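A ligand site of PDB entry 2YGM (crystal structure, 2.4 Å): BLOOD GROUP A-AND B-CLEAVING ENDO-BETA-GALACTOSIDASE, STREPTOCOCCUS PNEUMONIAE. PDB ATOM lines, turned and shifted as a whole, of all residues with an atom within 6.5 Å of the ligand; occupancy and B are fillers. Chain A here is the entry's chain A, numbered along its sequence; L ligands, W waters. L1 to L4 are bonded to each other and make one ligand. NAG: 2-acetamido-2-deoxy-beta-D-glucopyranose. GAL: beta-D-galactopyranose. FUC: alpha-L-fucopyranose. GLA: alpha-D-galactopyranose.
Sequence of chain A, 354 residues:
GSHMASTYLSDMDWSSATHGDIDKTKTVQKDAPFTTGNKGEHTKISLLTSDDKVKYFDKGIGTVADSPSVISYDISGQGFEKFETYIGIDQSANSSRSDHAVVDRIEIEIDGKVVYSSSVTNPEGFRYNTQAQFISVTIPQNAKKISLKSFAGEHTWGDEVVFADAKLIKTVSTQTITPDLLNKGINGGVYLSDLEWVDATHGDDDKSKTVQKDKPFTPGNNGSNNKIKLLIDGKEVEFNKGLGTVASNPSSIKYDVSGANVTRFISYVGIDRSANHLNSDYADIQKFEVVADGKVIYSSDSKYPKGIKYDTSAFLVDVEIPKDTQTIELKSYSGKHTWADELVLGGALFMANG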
ATOM      1  N   GLY A  20     -31.610  14.883  26.110  1.00  0.00           N
ATOM      2  CA  GLY A  20     -31.820  13.638  25.373  1.00  0.00           C
ATOM      3  C   GLY A  20     -30.568  12.964  24.830  1.00  0.00           C
ATOM      4  O   GLY A  20     -30.667  12.057  24.012  1.00  0.00           O
ATOM      5  N   ASP A  21     -29.393  13.414  25.266  1.00  0.00           N
ATOM      6  CA  ASP A  21     -28.145  12.756  24.877  1.00  0.00           C
ATOM      7  C   ASP A  21     -27.890  11.549  25.789  1.00  0.00           C
ATOM      8  O   ASP A  21     -28.067  11.642  27.004  1.00  0.00           O
ATOM      9  CB  ASP A  21     -26.965  13.732  24.953  1.00  0.00           C
ATOM     10  CG  ASP A  21     -25.816  13.321  24.055  1.00  0.00           C
ATOM     11  OD1 ASP A  21     -25.167  12.286  24.330  1.00  0.00           O
ATOM     12  OD2 ASP A  21     -25.548  14.046  23.072  1.00  0.00           O
ATOM     13  N   ILE A  22     -27.479  10.437  25.193  1.00  0.00           N
ATOM     14  CA  ILE A  22     -27.226   9.200  25.952  1.00  0.00           C
ATOM     15  C   ILE A  22     -26.099   9.353  26.989  1.00  0.00           C
ATOM     16  O   ILE A  22     -26.163   8.761  28.064  1.00  0.00           O
ATOM     17  CB  ILE A  22     -26.963   7.961  25.052  1.00  0.00           C
ATOM     18  CG1 ILE A  22     -26.215   8.333  23.761  1.00  0.00           C
ATOM     19  CG2 ILE A  22     -28.270   7.260  24.718  1.00  0.00           C
ATOM     20  CD1 ILE A  22     -24.707   8.233  23.861  1.00  0.00           C
ATOM     21  N   ASP A  23     -25.097  10.161  26.653  1.00  0.00           N
ATOM     22  CA  ASP A  23     -23.981  10.443  27.547  1.00  0.00           C
ATOM     23  C   ASP A  23     -24.429  11.354  28.691  1.00  0.00           C
ATOM     24  O   ASP A  23     -24.531  12.569  28.529  1.00  0.00           O
ATOM     25  CB  ASP A  23     -22.807  11.058  26.768  1.00  0.00           C
ATOM     26  CG  ASP A  23     -21.558  11.274  27.634  1.00  0.00           C
ATOM     27  OD1 ASP A  23     -21.597  11.018  28.849  1.00  0.00           O
ATOM     28  OD2 ASP A  23     -20.531  11.706  27.062  1.00  0.00           O
ATOM     29  N   LYS A  26     -22.365  14.472  30.210  1.00  0.00           N
ATOM     30  CA  LYS A  26     -22.641  15.766  29.604  1.00  0.00           C
ATOM     31  C   LYS A  26     -23.860  16.410  30.263  1.00  0.00           C
ATOM     32  O   LYS A  26     -24.764  15.713  30.732  1.00  0.00           O
ATOM     33  CB  LYS A  26     -22.901  15.598  28.099  1.00  0.00           C
ATOM     34  CG  LYS A  26     -21.739  15.018  27.329  1.00  0.00           C
ATOM     35  CD  LYS A  26     -22.142  14.728  25.895  1.00  0.00           C
ATOM     36  CE  LYS A  26     -20.944  14.334  25.056  1.00  0.00           C
ATOM     37  NZ  LYS A  26     -21.358  13.855  23.710  1.00  0.00           N
ATOM     38  N   PHE A  34     -25.554  22.630  22.814  1.00  0.00           N
ATOM     39  CA  PHE A  34     -25.332  21.492  23.689  1.00  0.00           C
ATOM     40  C   PHE A  34     -24.031  20.741  23.415  1.00  0.00           C
ATOM     41  O   PHE A  34     -23.238  20.525  24.333  1.00  0.00           O
ATOM     42  CB  PHE A  34     -26.519  20.520  23.672  1.00  0.00           C
ATOM     43  CG  PHE A  34     -26.440  19.453  24.728  1.00  0.00           C
ATOM     44  CD1 PHE A  34     -25.783  18.254  24.478  1.00  0.00           C
ATOM     45  CD2 PHE A  34     -27.019  19.656  25.979  1.00  0.00           C
ATOM     46  CE1 PHE A  34     -25.700  17.263  25.456  1.00  0.00           C
ATOM     47  CE2 PHE A  34     -26.945  18.676  26.960  1.00  0.00           C
ATOM     48  CZ  PHE A  34     -26.282  17.474  26.697  1.00  0.00           C
ATOM     49  N   THR A  35     -23.813  20.359  22.159  1.00  0.00           N
ATOM     50  CA  THR A  35     -22.671  19.517  21.790  1.00  0.00           C
ATOM     51  C   THR A  35     -21.357  20.300  21.802  1.00  0.00           C
ATOM     52  O   THR A  35     -20.376  19.854  22.419  1.00  0.00           O
ATOM     53  CB  THR A  35     -22.880  18.837  20.423  1.00  0.00           C
ATOM     54  OG1 THR A  35     -24.130  18.141  20.431  1.00  0.00           O
ATOM     55  CG2 THR A  35     -21.762  17.843  20.129  1.00  0.00           C
ATOM     56  N   THR A  36     -21.337  21.462  21.153  1.00  0.00           N
ATOM     57  CA  THR A  36     -20.139  22.313  21.097  1.00  0.00           C
ATOM     58  C   THR A  36     -19.718  22.781  22.487  1.00  0.00           C
ATOM     59  O   THR A  36     -18.526  22.860  22.793  1.00  0.00           O
ATOM     60  CB  THR A  36     -20.313  23.546  20.169  1.00  0.00           C
ATOM     61  OG1 THR A  36     -21.344  24.393  20.675  1.00  0.00           O
ATOM     62  CG2 THR A  36     -20.657  23.113  18.735  1.00  0.00           C
ATOM     63  N   LYS A  39     -18.167  19.886  24.417  1.00  0.00           N
ATOM     64  CA  LYS A  39     -16.851  19.655  23.806  1.00  0.00           C
ATOM     65  C   LYS A  39     -15.805  20.713  24.191  1.00  0.00           C
ATOM     66  O   LYS A  39     -14.622  20.534  23.927  1.00  0.00           O
ATOM     67  CB  LYS A  39     -16.967  19.585  22.276  1.00  0.00           C
ATOM     68  CG  LYS A  39     -17.470  18.246  21.748  1.00  0.00           C
ATOM     69  CD  LYS A  39     -17.285  18.143  20.246  1.00  0.00           C
ATOM     70  CE  LYS A  39     -17.957  16.895  19.699  1.00  0.00           C
ATOM     71  NZ  LYS A  39     -17.711  16.741  18.244  1.00  0.00           N
ATOM     72  N   VAL A  64     -30.588  19.200  24.430  1.00  0.00           N
ATOM     73  CA  VAL A  64     -31.020  18.209  23.458  1.00  0.00           C
ATOM     74  C   VAL A  64     -32.407  17.744  23.878  1.00  0.00           C
ATOM     75  O   VAL A  64     -32.613  17.370  25.033  1.00  0.00           O
ATOM     76  CB  VAL A  64     -30.040  17.005  23.374  1.00  0.00           C
ATOM     77  CG1 VAL A  64     -30.634  15.854  22.566  1.00  0.00           C
ATOM     78  CG2 VAL A  64     -28.709  17.442  22.767  1.00  0.00           C
ATOM     79  N   ALA A  65     -33.362  17.785  22.953  1.00  0.00           N
ATOM     80  CA  ALA A  65     -34.749  17.405  23.221  1.00  0.00           C
ATOM     81  C   ALA A  65     -34.854  15.925  23.611  1.00  0.00           C
ATOM     82  O   ALA A  65     -34.029  15.116  23.199  1.00  0.00           O
ATOM     83  CB  ALA A  65     -35.617  17.693  22.008  1.00  0.00           C
ATOM     84  N   ALA A  93     -26.104  22.215  14.680  1.00  0.00           N
ATOM     85  CA  ALA A  93     -26.632  20.863  14.784  1.00  0.00           C
ATOM     86  C   ALA A  93     -26.168  19.945  13.650  1.00  0.00           C
ATOM     87  O   ALA A  93     -26.145  20.339  12.486  1.00  0.00           O
ATOM     88  CB  ALA A  93     -28.158  20.902  14.823  1.00  0.00           C
ATOM     89  N   ASN A  94     -25.788  18.721  14.013  1.00  0.00           N
ATOM     90  CA  ASN A  94     -25.435  17.690  13.033  1.00  0.00           C
ATOM     91  C   ASN A  94     -26.687  17.275  12.253  1.00  0.00           C
ATOM     92  O   ASN A  94     -27.462  16.420  12.696  1.00  0.00           O
ATOM     93  CB  ASN A  94     -24.746  16.498  13.707  1.00  0.00           C
ATOM     94  CG  ASN A  94     -24.511  15.326  12.757  1.00  0.00           C
ATOM     95  OD1 ASN A  94     -24.081  15.507  11.618  1.00  0.00           O
ATOM     96  ND2 ASN A  94     -24.777  14.112  13.231  1.00  0.00           N
ATOM     97  N   ARG A  97     -28.293  14.002   8.124  1.00  0.00           N
ATOM     98  CA  ARG A  97     -29.345  13.001   8.017  1.00  0.00           C
ATOM     99  C   ARG A  97     -30.709  13.625   8.256  1.00  0.00           C
ATOM    100  O   ARG A  97     -30.882  14.445   9.165  1.00  0.00           O
ATOM    101  CB  ARG A  97     -29.110  11.864   9.001  1.00  0.00           C
ATOM    102  CG  ARG A  97     -28.066  10.841   8.552  1.00  0.00           C
ATOM    103  CD  ARG A  97     -27.615   9.956   9.703  1.00  0.00           C
ATOM    104  NE  ARG A  97     -28.661   9.060  10.180  1.00  0.00           N
ATOM    105  CZ  ARG A  97     -28.476   8.085  11.075  1.00  0.00           C
ATOM    106  NH1 ARG A  97     -27.270   7.879  11.589  1.00  0.00           N
ATOM    107  NH2 ARG A  97     -29.501   7.334  11.453  1.00  0.00           N
ATOM    108  N   HIS A 100     -32.232  13.487  11.645  1.00  0.00           N
ATOM    109  CA  HIS A 100     -31.581  14.333  12.637  1.00  0.00           C
ATOM    110  C   HIS A 100     -32.230  15.723  12.670  1.00  0.00           C
ATOM    111  O   HIS A 100     -32.846  16.146  11.688  1.00  0.00           O
ATOM    112  CB  HIS A 100     -30.088  14.480  12.323  1.00  0.00           C
ATOM    113  CG  HIS A 100     -29.241  13.365  12.840  1.00  0.00           C
ATOM    114  ND1 HIS A 100     -29.494  12.038  12.536  1.00  0.00           N
ATOM    115  CD2 HIS A 100     -28.143  13.362  13.626  1.00  0.00           C
ATOM    116  CE1 HIS A 100     -28.590  11.277  13.126  1.00  0.00           C
ATOM    117  NE2 HIS A 100     -27.759  12.067  13.792  1.00  0.00           N
ATOM    118  N   HIS A 155     -36.475  10.239  17.584  1.00  0.00           N
ATOM    119  CA  HIS A 155     -35.075  10.209  18.024  1.00  0.00           C
ATOM    120  C   HIS A 155     -34.660  11.556  18.606  1.00  0.00           C
ATOM    121  O   HIS A 155     -35.299  12.570  18.340  1.00  0.00           O
ATOM    122  CB  HIS A 155     -34.138   9.846  16.860  1.00  0.00           C
ATOM    123  CG  HIS A 155     -34.443   8.535  16.219  1.00  0.00           C
ATOM    124  ND1 HIS A 155     -33.971   7.340  16.706  1.00  0.00           N
ATOM    125  CD2 HIS A 155     -35.160   8.222  15.111  1.00  0.00           C
ATOM    126  CE1 HIS A 155     -34.392   6.352  15.938  1.00  0.00           C
ATOM    127  NE2 HIS A 155     -35.117   6.864  14.958  1.00  0.00           N
ATOM    128  N   THR A 156     -33.587  11.571  19.384  1.00  0.00           N
ATOM    129  CA  THR A 156     -33.067  12.810  19.957  1.00  0.00           C
ATOM    130  C   THR A 156     -31.971  13.413  19.065  1.00  0.00           C
ATOM    131  O   THR A 156     -31.450  14.497  19.353  1.00  0.00           O
ATOM    132  CB  THR A 156     -32.484  12.593  21.365  1.00  0.00           C
ATOM    133  OG1 THR A 156     -31.310  11.783  21.274  1.00  0.00           O
ATOM    134  CG2 THR A 156     -33.491  11.934  22.295  1.00  0.00           C
ATOM    135  N   TRP A 157     -31.638  12.709  17.984  1.00  0.00           N
ATOM    136  CA  TRP A 157     -30.479  13.029  17.171  1.00  0.00           C
ATOM    137  C   TRP A 157     -30.503  14.419  16.542  1.00  0.00           C
ATOM    138  O   TRP A 157     -31.438  14.768  15.808  1.00  0.00           O
ATOM    139  CB  TRP A 157     -30.277  11.957  16.097  1.00  0.00           C
ATOM    140  CG  TRP A 157     -30.069  10.562  16.654  1.00  0.00           C
ATOM    141  CD1 TRP A 157     -29.479  10.226  17.844  1.00  0.00           C
ATOM    142  CD2 TRP A 157     -30.443   9.320  16.039  1.00  0.00           C
ATOM    143  NE1 TRP A 157     -29.467   8.866  18.010  1.00  0.00           N
ATOM    144  CE2 TRP A 157     -30.053   8.285  16.915  1.00  0.00           C
ATOM    145  CE3 TRP A 157     -31.077   8.986  14.831  1.00  0.00           C
ATOM    146  CZ2 TRP A 157     -30.279   6.931  16.628  1.00  0.00           C
ATOM    147  CZ3 TRP A 157     -31.297   7.644  14.544  1.00  0.00           C
ATOM    148  CH2 TRP A 157     -30.894   6.634  15.438  1.00  0.00           C
ATOM    149  N   GLY A 158     -29.482  15.209  16.844  1.00  0.00           N
ATOM    150  CA  GLY A 158     -29.342  16.564  16.290  1.00  0.00           C
ATOM    151  C   GLY A 158     -30.345  17.570  16.808  1.00  0.00           C
ATOM    152  O   GLY A 158     -30.396  18.701  16.307  1.00  0.00           O
ATOM    153  N   ASP A 159     -31.136  17.186  17.813  1.00  0.00           N
ATOM    154  CA  ASP A 159     -32.160  18.045  18.383  1.00  0.00           C
ATOM    155  C   ASP A 159     -31.563  19.078  19.336  1.00  0.00           C
ATOM    156  O   ASP A 159     -31.947  19.170  20.502  1.00  0.00           O
ATOM    157  CB  ASP A 159     -33.234  17.214  19.095  1.00  0.00           C
ATOM    158  CG  ASP A 159     -34.004  16.321  18.146  1.00  0.00           C
ATOM    159  OD1 ASP A 159     -33.714  16.309  16.927  1.00  0.00           O
ATOM    160  OD2 ASP A 159     -34.921  15.615  18.611  1.00  0.00           O
ATOM    161  N   GLU A 160     -30.618  19.857  18.813  1.00  0.00           N
ATOM    162  CA  GLU A 160     -29.907  20.878  19.574  1.00  0.00           C
ATOM    163  C   GLU A 160     -30.790  22.100  19.826  1.00  0.00           C
ATOM    164  O   GLU A 160     -30.522  23.182  19.308  1.00  0.00           O
ATOM    165  CB  GLU A 160     -28.637  21.311  18.828  1.00  0.00           C
ATOM    166  CG  GLU A 160     -27.705  20.175  18.423  1.00  0.00           C
ATOM    167  CD  GLU A 160     -26.738  19.811  19.508  1.00  0.00           C
ATOM    168  OE1 GLU A 160     -26.054  20.720  20.026  1.00  0.00           O
ATOM    169  OE2 GLU A 160     -26.651  18.610  19.842  1.00  0.00           O
HETATM  170  C1  NAG L   1     -21.866   4.879  20.173  1.00  0.00           C
HETATM  171  C2  NAG L   1     -21.828   4.787  18.656  1.00  0.00           C
HETATM  172  C3  NAG L   1     -22.235   6.116  18.005  1.00  0.00           C
HETATM  173  C4  NAG L   1     -23.445   6.802  18.660  1.00  0.00           C
HETATM  174  C5  NAG L   1     -23.575   6.548  20.173  1.00  0.00           C
HETATM  175  C6  NAG L   1     -25.021   6.737  20.630  1.00  0.00           C
HETATM  176  C7  NAG L   1     -20.262   3.656  17.156  1.00  0.00           C
HETATM  177  C8  NAG L   1     -18.818   3.391  16.840  1.00  0.00           C
HETATM  178  N2  NAG L   1     -20.490   4.430  18.215  1.00  0.00           N
HETATM  179  O1  NAG L   1     -21.550   3.629  20.742  1.00  0.00           O
HETATM  180  O3  NAG L   1     -22.516   5.903  16.635  1.00  0.00           O
HETATM  181  O4  NAG L   1     -23.296   8.176  18.415  1.00  0.00           O
HETATM  182  O5  NAG L   1     -23.175   5.246  20.570  1.00  0.00           O
HETATM  183  O6  NAG L   1     -25.851   5.698  20.158  1.00  0.00           O
HETATM  184  O7  NAG L   1     -21.149   3.154  16.468  1.00  0.00           O
HETATM  185  C1  GAL L   2     -24.523   8.795  17.982  1.00  0.00           C
HETATM  186  C2  GAL L   2     -24.392  10.308  18.104  1.00  0.00           C
HETATM  187  C3  GAL L   2     -25.646  11.047  17.618  1.00  0.00           C
HETATM  188  C4  GAL L   2     -26.268  10.413  16.367  1.00  0.00           C
HETATM  189  C5  GAL L   2     -26.251   8.880  16.428  1.00  0.00           C
HETATM  190  C6  GAL L   2     -26.786   8.223  15.158  1.00  0.00           C
HETATM  191  O2  GAL L   2     -24.154  10.580  19.466  1.00  0.00           O
HETATM  192  O3  GAL L   2     -25.242  12.385  17.372  1.00  0.00           O
HETATM  193  O4  GAL L   2     -25.621  10.885  15.206  1.00  0.00           O
HETATM  194  O5  GAL L   2     -24.930   8.437  16.678  1.00  0.00           O
HETATM  195  O6  GAL L   2     -26.915   6.839  15.382  1.00  0.00           O
HETATM  196  C1  FUC L   3     -23.106  11.551  19.689  1.00  0.00           C
HETATM  197  C2  FUC L   3     -23.224  12.074  21.120  1.00  0.00           C
HETATM  198  C3  FUC L   3     -22.766  11.008  22.113  1.00  0.00           C
HETATM  199  C4  FUC L   3     -21.352  10.548  21.784  1.00  0.00           C
HETATM  200  C5  FUC L   3     -21.314  10.061  20.325  1.00  0.00           C
HETATM  201  C6  FUC L   3     -19.932   9.583  19.905  1.00  0.00           C
HETATM  202  O2  FUC L   3     -24.568  12.411  21.380  1.00  0.00           O
HETATM  203  O3  FUC L   3     -22.839  11.511  23.426  1.00  0.00           O
HETATM  204  O4  FUC L   3     -20.448  11.608  21.961  1.00  0.00           O
HETATM  205  O5  FUC L   3     -21.781  11.084  19.447  1.00  0.00           O
HETATM  206  C1  GLA L   4     -26.279  13.406  17.364  1.00  0.00           C
HETATM  207  C2  GLA L   4     -25.583  14.768  17.296  1.00  0.00           C
HETATM  208  C3  GLA L   4     -25.049  15.162  18.667  1.00  0.00           C
HETATM  209  C4  GLA L   4     -26.183  15.179  19.684  1.00  0.00           C
HETATM  210  C5  GLA L   4     -26.878  13.825  19.712  1.00  0.00           C
HETATM  211  C6  GLA L   4     -28.098  13.857  20.631  1.00  0.00           C
HETATM  212  O2  GLA L   4     -24.513  14.733  16.380  1.00  0.00           O
HETATM  213  O3  GLA L   4     -24.435  16.429  18.604  1.00  0.00           O
HETATM  214  O4  GLA L   4     -27.111  16.199  19.347  1.00  0.00           O
HETATM  215  O5  GLA L   4     -27.262  13.386  18.412  1.00  0.00           O
HETATM  216  O6  GLA L   4     -28.852  12.669  20.502  1.00  0.00           O
HETATM  217  O   HOH W   1     -23.739   3.218  22.674  1.00  0.00           O
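The side-chain carboxylate of Glu 160 is in hydrogen-bond range of an oxygen (O4) of GLA L4 (2.5 Å). The side-chain hydroxyl of Thr 35 lies within hydrogen-bond range of an oxygen (O3) of GLA L4. OD2 of Asp 21 lies within hydrogen-bond range of O2 of FUC L3 (2.5 Å). O of Thr 156 is in hydrogen-bond range of O6 of GLA L4. O6 of GLA L4 is in hydrogen-bond range of OG1 of Thr 156. The side-chain amino group (NZ) of Lys 26 lies within hydrogen-bond range of an oxygen (O3) of FUC L3 (2.8 Å). O4 of GAL L2 lies within hydrogen-bond range of NE2 of His 100, 2.8 Å away. The side-chain amide nitrogen (ND2) of Asn 94 sits close to an oxygen (O2) of GLA L4 (3.2 Å). The backbone NH (N) of Gly 158 lies within hydrogen-bond range of an oxygen (O5) of GLA L4, at 3.3 Å.
The side-chain hydroxyl (OG1) of Thr 35 is in hydrogen-bond range of the side-chain carboxylate (OE2) of Glu 160, 2.6 Å away. N of Phe 34 is in hydrogen-bond range of OE1 of Glu 160 (3.4 Å). The side-chain carboxylate of Asp 21 is in hydrogen-bond range of the backbone NH of Asp 23, at 3.1 Å. OG1 of Thr 156 is in hydrogen-bond range of O of Gly 20 (2.8 Å). The backbone NH (N) of Gly 20 sits at hydrogen-bond distance from the backbone carbonyl oxygen (O) of Val 64.
O of Gly 20 touches O6 of GLA L4, 3.999 Å away. CD1 of Ile 22 touches C6 of NAG L1, 3.6 Å away. Asp 23 touches the ligand. CG1 of Val 64 touches C6 of GLA L4 (3.8 Å). NH1 of Arg 97 touches C6 of GAL L2, 3.6 Å away. CA of Trp 157 touches O5 of GLA L4, at 3.5 Å. Within 4 Å of the ligand: Gly 20, Asp 21, Ile 22, Asp 23, Lys 26, Thr 35, Val 64, Asn 94, Arg 97, His 100, Thr 156, Trp 157, Gly 158 and Glu 160.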
